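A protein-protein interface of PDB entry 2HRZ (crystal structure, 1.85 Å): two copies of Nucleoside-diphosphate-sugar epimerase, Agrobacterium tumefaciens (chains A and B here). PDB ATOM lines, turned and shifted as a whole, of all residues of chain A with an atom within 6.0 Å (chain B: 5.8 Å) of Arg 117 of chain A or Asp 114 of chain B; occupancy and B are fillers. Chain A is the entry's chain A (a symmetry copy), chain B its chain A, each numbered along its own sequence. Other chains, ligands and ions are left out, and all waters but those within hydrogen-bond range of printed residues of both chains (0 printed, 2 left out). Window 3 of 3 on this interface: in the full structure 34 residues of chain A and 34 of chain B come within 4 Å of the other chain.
The side-chain carboxylate (OD1) of Asp 114 of chain B is in salt-bridge range of the guanidinium group (NH2) of Arg 117 of chain A. The guanidinium group of Arg 117 of chain B is in salt-bridge range of the side-chain carboxylate of Asp 114 of chain A (3.0 Å).
The backbone carbonyl oxygen (O) of Tyr 109 of chain B lies within hydrogen-bond range of the backbone NH (N) of Asp 114 of chain B (2.9 Å). The guanidinium group (NE) of Arg 117 of chain A lies within salt-bridge range of the side-chain carboxylate (OD2) of Asp 121 of chain A (3.3 Å).
Arg 117 of chain B touches Leu 113 of chain A. Tyr 109 of chain B touches Arg 117 of chain A (CB to NH1, 3.9 Å). Leu 113 of chain B touches Arg 117 of chain A. Leu 175 of chain A touches Tyr 109 of chain B (CD2 to CE2, 3.7 Å).
Leu 113 of chain A touches Arg 117 of chain B, and with the chains exchanged Arg 117 of chain A touches Leu 113 of chain B. Asp 114 of chain A touches Arg 117 of chain B, and with the chains exchanged Arg 117 of chain A touches Asp 114 of chain B. 7 positions are printed for both chains. Of the 6 pairs that touch across the chains among the printed residues, 4 have their exchanged pair printed and touching as well.
Printed residues of chain B within 4 Å of Leu 113 of chain A: Arg 117 (3.8 Å). Of the printed residues of chain B, Asp 114 of chain A touches Arg 117. Arg 117 of chain A touches just these residues of chain B: Tyr 109, Leu 113 and Asp 114. Of the printed residues of chain B, Leu 175 of chain A touches Tyr 109 (3.7 Å). Tyr 179 of chain A touches none of the printed residues of chain B. Of the printed residues of chain A, Tyr 109 of chain B touches Arg 117 (3.9 Å) and Leu 175 (3.7 Å). Of chain A, only Arg 117 (3.0 Å) comes within 4 Å of Asp 114 of chain B. Printed residues of chain A within 4 Å of Arg 117 of chain B: Leu 113 (3.8 Å) and Asp 114 (3.0 Å). The nearest residue of chain B that does not touch Arg 117 of chain A is Arg 110 of chain B (5.3 Å). The nearest printed residue of chain A that does not touch Asp 114 of chain B is Asp 121 of chain A (7.0 Å).
Printed residues of chain B that touch a printed residue of chain A: Tyr 109, Leu 113, Asp 114 and Arg 117. Among the printed residues, 6 pairs touch across the chains. Among the printed residues, Asp or Glu carboxylates within 4 Å of a Lys or Arg side-chain nitrogen of the other chain: Asp 114 of chain A with Arg 117 of chain B (3.0 Å) and Arg 117 of chain A with Asp 114 of chain B (3.0 Å).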
ATOM      1  N   LEU A 113       7.462   3.921 -24.960  1.00  0.00           N
ATOM      2  CA  LEU A 113       7.859   4.981 -24.040  1.00  0.00           C
ATOM      3  C   LEU A 113       6.771   5.262 -23.005  1.00  0.00           C
ATOM      4  O   LEU A 113       7.000   5.082 -21.799  1.00  0.00           O
ATOM      5  CB  LEU A 113       8.271   6.277 -24.779  1.00  0.00           C
ATOM      6  CG  LEU A 113       8.577   7.518 -23.921  1.00  0.00           C
ATOM      7  CD1 LEU A 113       9.585   7.190 -22.807  1.00  0.00           C
ATOM      8  CD2 LEU A 113       9.087   8.721 -24.799  1.00  0.00           C
ATOM      9  N   ASP A 114       5.605   5.713 -23.466  1.00  0.00           N
ATOM     10  CA  ASP A 114       4.560   6.178 -22.554  1.00  0.00           C
ATOM     11  C   ASP A 114       4.126   5.114 -21.551  1.00  0.00           C
ATOM     12  O   ASP A 114       3.996   5.408 -20.357  1.00  0.00           O
ATOM     13  CB  ASP A 114       3.359   6.736 -23.329  1.00  0.00           C
ATOM     14  CG  ASP A 114       3.700   8.017 -24.095  1.00  0.00           C
ATOM     15  OD1 ASP A 114       4.748   8.636 -23.803  1.00  0.00           O
ATOM     16  OD2 ASP A 114       2.917   8.404 -24.980  1.00  0.00           O
ATOM     17  N   GLY A 115       3.933   3.883 -22.026  1.00  0.00           N
ATOM     18  CA  GLY A 115       3.519   2.757 -21.161  1.00  0.00           C
ATOM     19  C   GLY A 115       4.538   2.493 -20.060  1.00  0.00           C
ATOM     20  O   GLY A 115       4.178   2.269 -18.903  1.00  0.00           O
ATOM     21  N   THR A 116       5.813   2.553 -20.426  1.00  0.00           N
ATOM     22  CA  THR A 116       6.900   2.429 -19.453  1.00  0.00           C
ATOM     23  C   THR A 116       6.883   3.582 -18.455  1.00  0.00           C
ATOM     24  O   THR A 116       6.990   3.360 -17.242  1.00  0.00           O
ATOM     25  CB  THR A 116       8.245   2.358 -20.164  1.00  0.00           C
ATOM     26  OG1 THR A 116       8.227   1.244 -21.063  1.00  0.00           O
ATOM     27  CG2 THR A 116       9.368   2.188 -19.151  1.00  0.00           C
ATOM     28  N   ARG A 117       6.754   4.810 -18.957  1.00  0.00           N
ATOM     29  CA  ARG A 117       6.631   5.967 -18.085  1.00  0.00           C
ATOM     30  C   ARG A 117       5.443   5.803 -17.123  1.00  0.00           C
ATOM     31  O   ARG A 117       5.584   6.035 -15.921  1.00  0.00           O
ATOM     32  CB  ARG A 117       6.520   7.259 -18.910  1.00  0.00           C
ATOM     33  CG  ARG A 117       6.245   8.506 -18.077  1.00  0.00           C
ATOM     34  CD  ARG A 117       7.484   9.327 -17.843  1.00  0.00           C
ATOM     35  NE  ARG A 117       7.186  10.574 -17.124  1.00  0.00           N
ATOM     36  CZ  ARG A 117       6.962  11.759 -17.697  1.00  0.00           C
ATOM     37  NH1 ARG A 117       6.707  12.818 -16.942  1.00  0.00           N
ATOM     38  NH2 ARG A 117       6.971  11.896 -19.011  1.00  0.00           N
ATOM     39  N   TYR A 118       4.282   5.386 -17.638  1.00  0.00           N
ATOM     40  CA  TYR A 118       3.118   5.169 -16.773  1.00  0.00           C
ATOM     41  C   TYR A 118       3.407   4.156 -15.656  1.00  0.00           C
ATOM     42  O   TYR A 118       3.020   4.380 -14.517  1.00  0.00           O
ATOM     43  CB  TYR A 118       1.898   4.681 -17.556  1.00  0.00           C
ATOM     44  CG  TYR A 118       1.415   5.614 -18.641  1.00  0.00           C
ATOM     45  CD1 TYR A 118       1.754   6.978 -18.641  1.00  0.00           C
ATOM     46  CD2 TYR A 118       0.593   5.137 -19.662  1.00  0.00           C
ATOM     47  CE1 TYR A 118       1.302   7.835 -19.650  1.00  0.00           C
ATOM     48  CE2 TYR A 118       0.133   5.978 -20.658  1.00  0.00           C
ATOM     49  CZ  TYR A 118       0.490   7.321 -20.653  1.00  0.00           C
ATOM     50  OH  TYR A 118       0.030   8.131 -21.662  1.00  0.00           O
ATOM     51  N   LEU A 119       4.067   3.054 -15.998  1.00  0.00           N
ATOM     52  CA  LEU A 119       4.460   2.052 -15.008  1.00  0.00           C
ATOM     53  C   LEU A 119       5.376   2.673 -13.956  1.00  0.00           C
ATOM     54  O   LEU A 119       5.152   2.509 -12.773  1.00  0.00           O
ATOM     55  CB  LEU A 119       5.182   0.881 -15.671  1.00  0.00           C
ATOM     56  CG  LEU A 119       5.789  -0.172 -14.720  1.00  0.00           C
ATOM     57  CD1 LEU A 119       4.696  -0.927 -13.924  1.00  0.00           C
ATOM     58  CD2 LEU A 119       6.658  -1.126 -15.509  1.00  0.00           C
ATOM     59  N   PHE A 120       6.409   3.380 -14.404  1.00  0.00           N
ATOM     60  CA  PHE A 120       7.389   3.964 -13.495  1.00  0.00           C
ATOM     61  C   PHE A 120       6.732   4.978 -12.552  1.00  0.00           C
ATOM     62  O   PHE A 120       7.013   4.986 -11.347  1.00  0.00           O
ATOM     63  CB  PHE A 120       8.525   4.617 -14.287  1.00  0.00           C
ATOM     64  CG  PHE A 120       9.487   3.634 -14.932  1.00  0.00           C
ATOM     65  CD1 PHE A 120       9.284   2.251 -14.861  1.00  0.00           C
ATOM     66  CD2 PHE A 120      10.588   4.111 -15.647  1.00  0.00           C
ATOM     67  CE1 PHE A 120      10.177   1.357 -15.447  1.00  0.00           C
ATOM     68  CE2 PHE A 120      11.485   3.233 -16.262  1.00  0.00           C
ATOM     69  CZ  PHE A 120      11.288   1.860 -16.177  1.00  0.00           C
ATOM     70  N   ASP A 121       5.846   5.819 -13.104  1.00  0.00           N
ATOM     71  CA  ASP A 121       5.115   6.768 -12.281  1.00  0.00           C
ATOM     72  C   ASP A 121       4.138   6.107 -11.302  1.00  0.00           C
ATOM     73  O   ASP A 121       3.996   6.578 -10.185  1.00  0.00           O
ATOM     74  CB  ASP A 121       4.429   7.844 -13.137  1.00  0.00           C
ATOM     75  CG  ASP A 121       5.394   8.932 -13.572  1.00  0.00           C
ATOM     76  OD1 ASP A 121       6.255   9.328 -12.753  1.00  0.00           O
ATOM     77  OD2 ASP A 121       5.281   9.404 -14.732  1.00  0.00           O
ATOM     78  N   ALA A 122       3.471   5.031 -11.713  1.00  0.00           N
ATOM     79  CA  ALA A 122       2.560   4.326 -10.795  1.00  0.00           C
ATOM     80  C   ALA A 122       3.347   3.749  -9.612  1.00  0.00           C
ATOM     81  O   ALA A 122       2.901   3.834  -8.450  1.00  0.00           O
ATOM     82  CB  ALA A 122       1.779   3.230 -11.512  1.00  0.00           C
ATOM     83  N   CYS A 172      13.807   5.219 -21.888  1.00  0.00           N
ATOM     84  CA  CYS A 172      13.377   4.373 -20.756  1.00  0.00           C
ATOM     85  C   CYS A 172      14.560   4.078 -19.824  1.00  0.00           C
ATOM     86  O   CYS A 172      14.428   4.126 -18.602  1.00  0.00           O
ATOM     87  CB  CYS A 172      12.772   3.066 -21.274  1.00  0.00           C
ATOM     88  SG  CYS A 172      11.131   3.267 -22.025  1.00  0.00           S
ATOM     89  N   LEU A 175      15.107   7.171 -17.629  1.00  0.00           N
ATOM     90  CA  LEU A 175      14.056   7.227 -16.610  1.00  0.00           C
ATOM     91  C   LEU A 175      14.322   6.183 -15.518  1.00  0.00           C
ATOM     92  O   LEU A 175      14.211   6.470 -14.323  1.00  0.00           O
ATOM     93  CB  LEU A 175      12.673   6.986 -17.232  1.00  0.00           C
ATOM     94  CG  LEU A 175      12.151   8.115 -18.139  1.00  0.00           C
ATOM     95  CD1 LEU A 175      10.900   7.630 -18.902  1.00  0.00           C
ATOM     96  CD2 LEU A 175      11.838   9.369 -17.319  1.00  0.00           C
ATOM     97  N   TYR A 179      14.685   7.293 -11.591  1.00  0.00           N
ATOM     98  CA  TYR A 179      13.726   6.784 -10.592  1.00  0.00           C
ATOM     99  C   TYR A 179      14.393   5.882  -9.559  1.00  0.00           C
ATOM    100  O   TYR A 179      14.024   5.901  -8.372  1.00  0.00           O
ATOM    101  CB  TYR A 179      12.595   6.024 -11.278  1.00  0.00           C
ATOM    102  CG  TYR A 179      11.553   6.918 -11.935  1.00  0.00           C
ATOM    103  CD1 TYR A 179      11.919   7.887 -12.896  1.00  0.00           C
ATOM    104  CD2 TYR A 179      10.197   6.772 -11.626  1.00  0.00           C
ATOM    105  CE1 TYR A 179      10.936   8.706 -13.520  1.00  0.00           C
ATOM    106  CE2 TYR A 179       9.223   7.558 -12.238  1.00  0.00           C
ATOM    107  CZ  TYR A 179       9.596   8.528 -13.182  1.00  0.00           C
ATOM    108  OH  TYR A 179       8.610   9.300 -13.778  1.00  0.00           O
ATOM    109  N   SER B  74       4.350  23.987 -20.907  1.00  0.00           N
ATOM    110  CA  SER B  74       3.745  22.727 -20.431  1.00  0.00           C
ATOM    111  C   SER B  74       2.228  22.823 -20.248  1.00  0.00           C
ATOM    112  O   SER B  74       1.537  21.801 -20.119  1.00  0.00           O
ATOM    113  CB  SER B  74       4.416  22.241 -19.131  1.00  0.00           C
ATOM    114  OG  SER B  74       4.100  23.081 -18.029  1.00  0.00           O
ATOM    115  N   GLY B 108       9.729  19.539 -12.204  1.00  0.00           N
ATOM    116  CA  GLY B 108      10.845  19.356 -13.126  1.00  0.00           C
ATOM    117  C   GLY B 108      10.480  18.524 -14.349  1.00  0.00           C
ATOM    118  O   GLY B 108      10.760  18.925 -15.484  1.00  0.00           O
ATOM    119  N   TYR B 109       9.865  17.365 -14.134  1.00  0.00           N
ATOM    120  CA  TYR B 109       9.473  16.531 -15.276  1.00  0.00           C
ATOM    121  C   TYR B 109       8.429  17.201 -16.150  1.00  0.00           C
ATOM    122  O   TYR B 109       8.478  17.078 -17.364  1.00  0.00           O
ATOM    123  CB  TYR B 109       9.024  15.135 -14.851  1.00  0.00           C
ATOM    124  CG  TYR B 109      10.212  14.207 -14.721  1.00  0.00           C
ATOM    125  CD1 TYR B 109      10.843  14.013 -13.494  1.00  0.00           C
ATOM    126  CD2 TYR B 109      10.736  13.577 -15.850  1.00  0.00           C
ATOM    127  CE1 TYR B 109      11.993  13.171 -13.389  1.00  0.00           C
ATOM    128  CE2 TYR B 109      11.840  12.743 -15.765  1.00  0.00           C
ATOM    129  CZ  TYR B 109      12.476  12.552 -14.545  1.00  0.00           C
ATOM    130  OH  TYR B 109      13.563  11.717 -14.512  1.00  0.00           O
ATOM    131  N   ARG B 110       7.488  17.899 -15.529  1.00  0.00           N
ATOM    132  CA  ARG B 110       6.458  18.628 -16.285  1.00  0.00           C
ATOM    133  C   ARG B 110       7.087  19.694 -17.187  1.00  0.00           C
ATOM    134  O   ARG B 110       6.815  19.740 -18.390  1.00  0.00           O
ATOM    135  CB  ARG B 110       5.436  19.286 -15.332  1.00  0.00           C
ATOM    136  CG  ARG B 110       4.387  20.124 -16.074  1.00  0.00           C
ATOM    137  CD  ARG B 110       3.188  20.478 -15.177  1.00  0.00           C
ATOM    138  NE  ARG B 110       3.552  21.285 -14.014  1.00  0.00           N
ATOM    139  CZ  ARG B 110       3.799  22.596 -14.033  1.00  0.00           C
ATOM    140  NH1 ARG B 110       3.760  23.292 -15.169  1.00  0.00           N
ATOM    141  NH2 ARG B 110       4.092  23.213 -12.897  1.00  0.00           N
ATOM    142  N   ILE B 111       7.918  20.550 -16.599  1.00  0.00           N
ATOM    143  CA  ILE B 111       8.475  21.695 -17.347  1.00  0.00           C
ATOM    144  C   ILE B 111       9.652  21.322 -18.253  1.00  0.00           C
ATOM    145  O   ILE B 111       9.718  21.764 -19.407  1.00  0.00           O
ATOM    146  CB  ILE B 111       8.811  22.875 -16.402  1.00  0.00           C
ATOM    147  CG1 ILE B 111       7.494  23.512 -15.923  1.00  0.00           C
ATOM    148  CG2 ILE B 111       9.734  23.935 -17.097  1.00  0.00           C
ATOM    149  CD1 ILE B 111       7.568  24.214 -14.608  1.00  0.00           C
ATOM    150  N   ASN B 112      10.565  20.503 -17.753  1.00  0.00           N
ATOM    151  CA  ASN B 112      11.788  20.203 -18.511  1.00  0.00           C
ATOM    152  C   ASN B 112      11.658  19.063 -19.520  1.00  0.00           C
ATOM    153  O   ASN B 112      12.432  19.008 -20.485  1.00  0.00           O
ATOM    154  CB  ASN B 112      12.969  19.957 -17.577  1.00  0.00           C
ATOM    155  CG  ASN B 112      13.275  21.154 -16.702  1.00  0.00           C
ATOM    156  OD1 ASN B 112      12.821  22.254 -16.979  1.00  0.00           O
ATOM    157  ND2 ASN B 112      14.019  20.938 -15.621  1.00  0.00           N
ATOM    158  N   LEU B 113      10.738  18.134 -19.280  1.00  0.00           N
ATOM    159  CA  LEU B 113      10.521  17.041 -20.221  1.00  0.00           C
ATOM    160  C   LEU B 113       9.202  17.202 -20.975  1.00  0.00           C
ATOM    161  O   LEU B 113       9.204  17.339 -22.208  1.00  0.00           O
ATOM    162  CB  LEU B 113      10.607  15.654 -19.540  1.00  0.00           C
ATOM    163  CG  LEU B 113      10.258  14.420 -20.393  1.00  0.00           C
ATOM    164  CD1 LEU B 113      11.041  14.420 -21.716  1.00  0.00           C
ATOM    165  CD2 LEU B 113      10.495  13.080 -19.603  1.00  0.00           C
ATOM    166  N   ASP B 114       8.086  17.170 -20.247  1.00  0.00           N
ATOM    167  CA  ASP B 114       6.769  17.139 -20.883  1.00  0.00           C
ATOM    168  C   ASP B 114       6.523  18.329 -21.806  1.00  0.00           C
ATOM    169  O   ASP B 114       6.036  18.149 -22.927  1.00  0.00           O
ATOM    170  CB  ASP B 114       5.655  17.006 -19.836  1.00  0.00           C
ATOM    171  CG  ASP B 114       5.687  15.657 -19.114  1.00  0.00           C
ATOM    172  OD1 ASP B 114       6.357  14.722 -19.607  1.00  0.00           O
ATOM    173  OD2 ASP B 114       5.036  15.533 -18.061  1.00  0.00           O
ATOM    174  N   GLY B 115       6.886  19.528 -21.351  1.00  0.00           N
ATOM    175  CA  GLY B 115       6.712  20.763 -22.147  1.00  0.00           C
ATOM    176  C   GLY B 115       7.485  20.697 -23.457  1.00  0.00           C
ATOM    177  O   GLY B 115       6.978  21.081 -24.513  1.00  0.00           O
ATOM    178  N   THR B 116       8.705  20.179 -23.383  1.00  0.00           N
ATOM    179  CA  THR B 116       9.520  19.952 -24.579  1.00  0.00           C
ATOM    180  C   THR B 116       8.877  18.922 -25.499  1.00  0.00           C
ATOM    181  O   THR B 116       8.781  19.141 -26.714  1.00  0.00           O
ATOM    182  CB  THR B 116      10.927  19.519 -24.190  1.00  0.00           C
ATOM    183  OG1 THR B 116      11.501  20.530 -23.356  1.00  0.00           O
ATOM    184  CG2 THR B 116      11.783  19.325 -25.434  1.00  0.00           C
ATOM    185  N   ARG B 117       8.441  17.797 -24.931  1.00  0.00           N
ATOM    186  CA  ARG B 117       7.729  16.793 -25.706  1.00  0.00           C
ATOM    187  C   ARG B 117       6.491  17.403 -26.384  1.00  0.00           C
ATOM    188  O   ARG B 117       6.269  17.186 -27.576  1.00  0.00           O
ATOM    189  CB  ARG B 117       7.359  15.590 -24.824  1.00  0.00           C
ATOM    190  CG  ARG B 117       6.486  14.554 -25.523  1.00  0.00           C
ATOM    191  CD  ARG B 117       7.272  13.360 -25.994  1.00  0.00           C
ATOM    192  NE  ARG B 117       6.403  12.328 -26.576  1.00  0.00           N
ATOM    193  CZ  ARG B 117       5.911  11.275 -25.920  1.00  0.00           C
ATOM    194  NH1 ARG B 117       5.139  10.405 -26.554  1.00  0.00           N
ATOM    195  NH2 ARG B 117       6.165  11.090 -24.636  1.00  0.00           N
ATOM    196  N   TYR B 118       5.697  18.180 -25.640  1.00  0.00           N
ATOM    197  CA  TYR B 118       4.521  18.827 -26.232  1.00  0.00           C
ATOM    198  C   TYR B 118       4.890  19.718 -27.425  1.00  0.00           C
ATOM    199  O   TYR B 118       4.205  19.692 -28.439  1.00  0.00           O
ATOM    200  CB  TYR B 118       3.758  19.679 -25.217  1.00  0.00           C
ATOM    201  CG  TYR B 118       3.233  18.931 -24.014  1.00  0.00           C
ATOM    202  CD1 TYR B 118       3.063  17.536 -24.033  1.00  0.00           C
ATOM    203  CD2 TYR B 118       2.881  19.624 -22.855  1.00  0.00           C
ATOM    204  CE1 TYR B 118       2.576  16.852 -22.915  1.00  0.00           C
ATOM    205  CE2 TYR B 118       2.390  18.958 -21.748  1.00  0.00           C
ATOM    206  CZ  TYR B 118       2.243  17.576 -21.778  1.00  0.00           C
ATOM    207  OH  TYR B 118       1.766  16.939 -20.660  1.00  0.00           O
ATOM    208  N   LEU B 119       5.954  20.505 -27.285  1.00  0.00           N
ATOM    209  CA  LEU B 119       6.441  21.344 -28.378  1.00  0.00           C
ATOM    210  C   LEU B 119       6.821  20.485 -29.581  1.00  0.00           C
ATOM    211  O   LEU B 119       6.410  20.766 -30.690  1.00  0.00           O
ATOM    212  CB  LEU B 119       7.656  22.159 -27.941  1.00  0.00           C
ATOM    213  CG  LEU B 119       8.365  22.970 -29.047  1.00  0.00           C
ATOM    214  CD1 LEU B 119       7.458  24.092 -29.609  1.00  0.00           C
ATOM    215  CD2 LEU B 119       9.666  23.526 -28.511  1.00  0.00           C
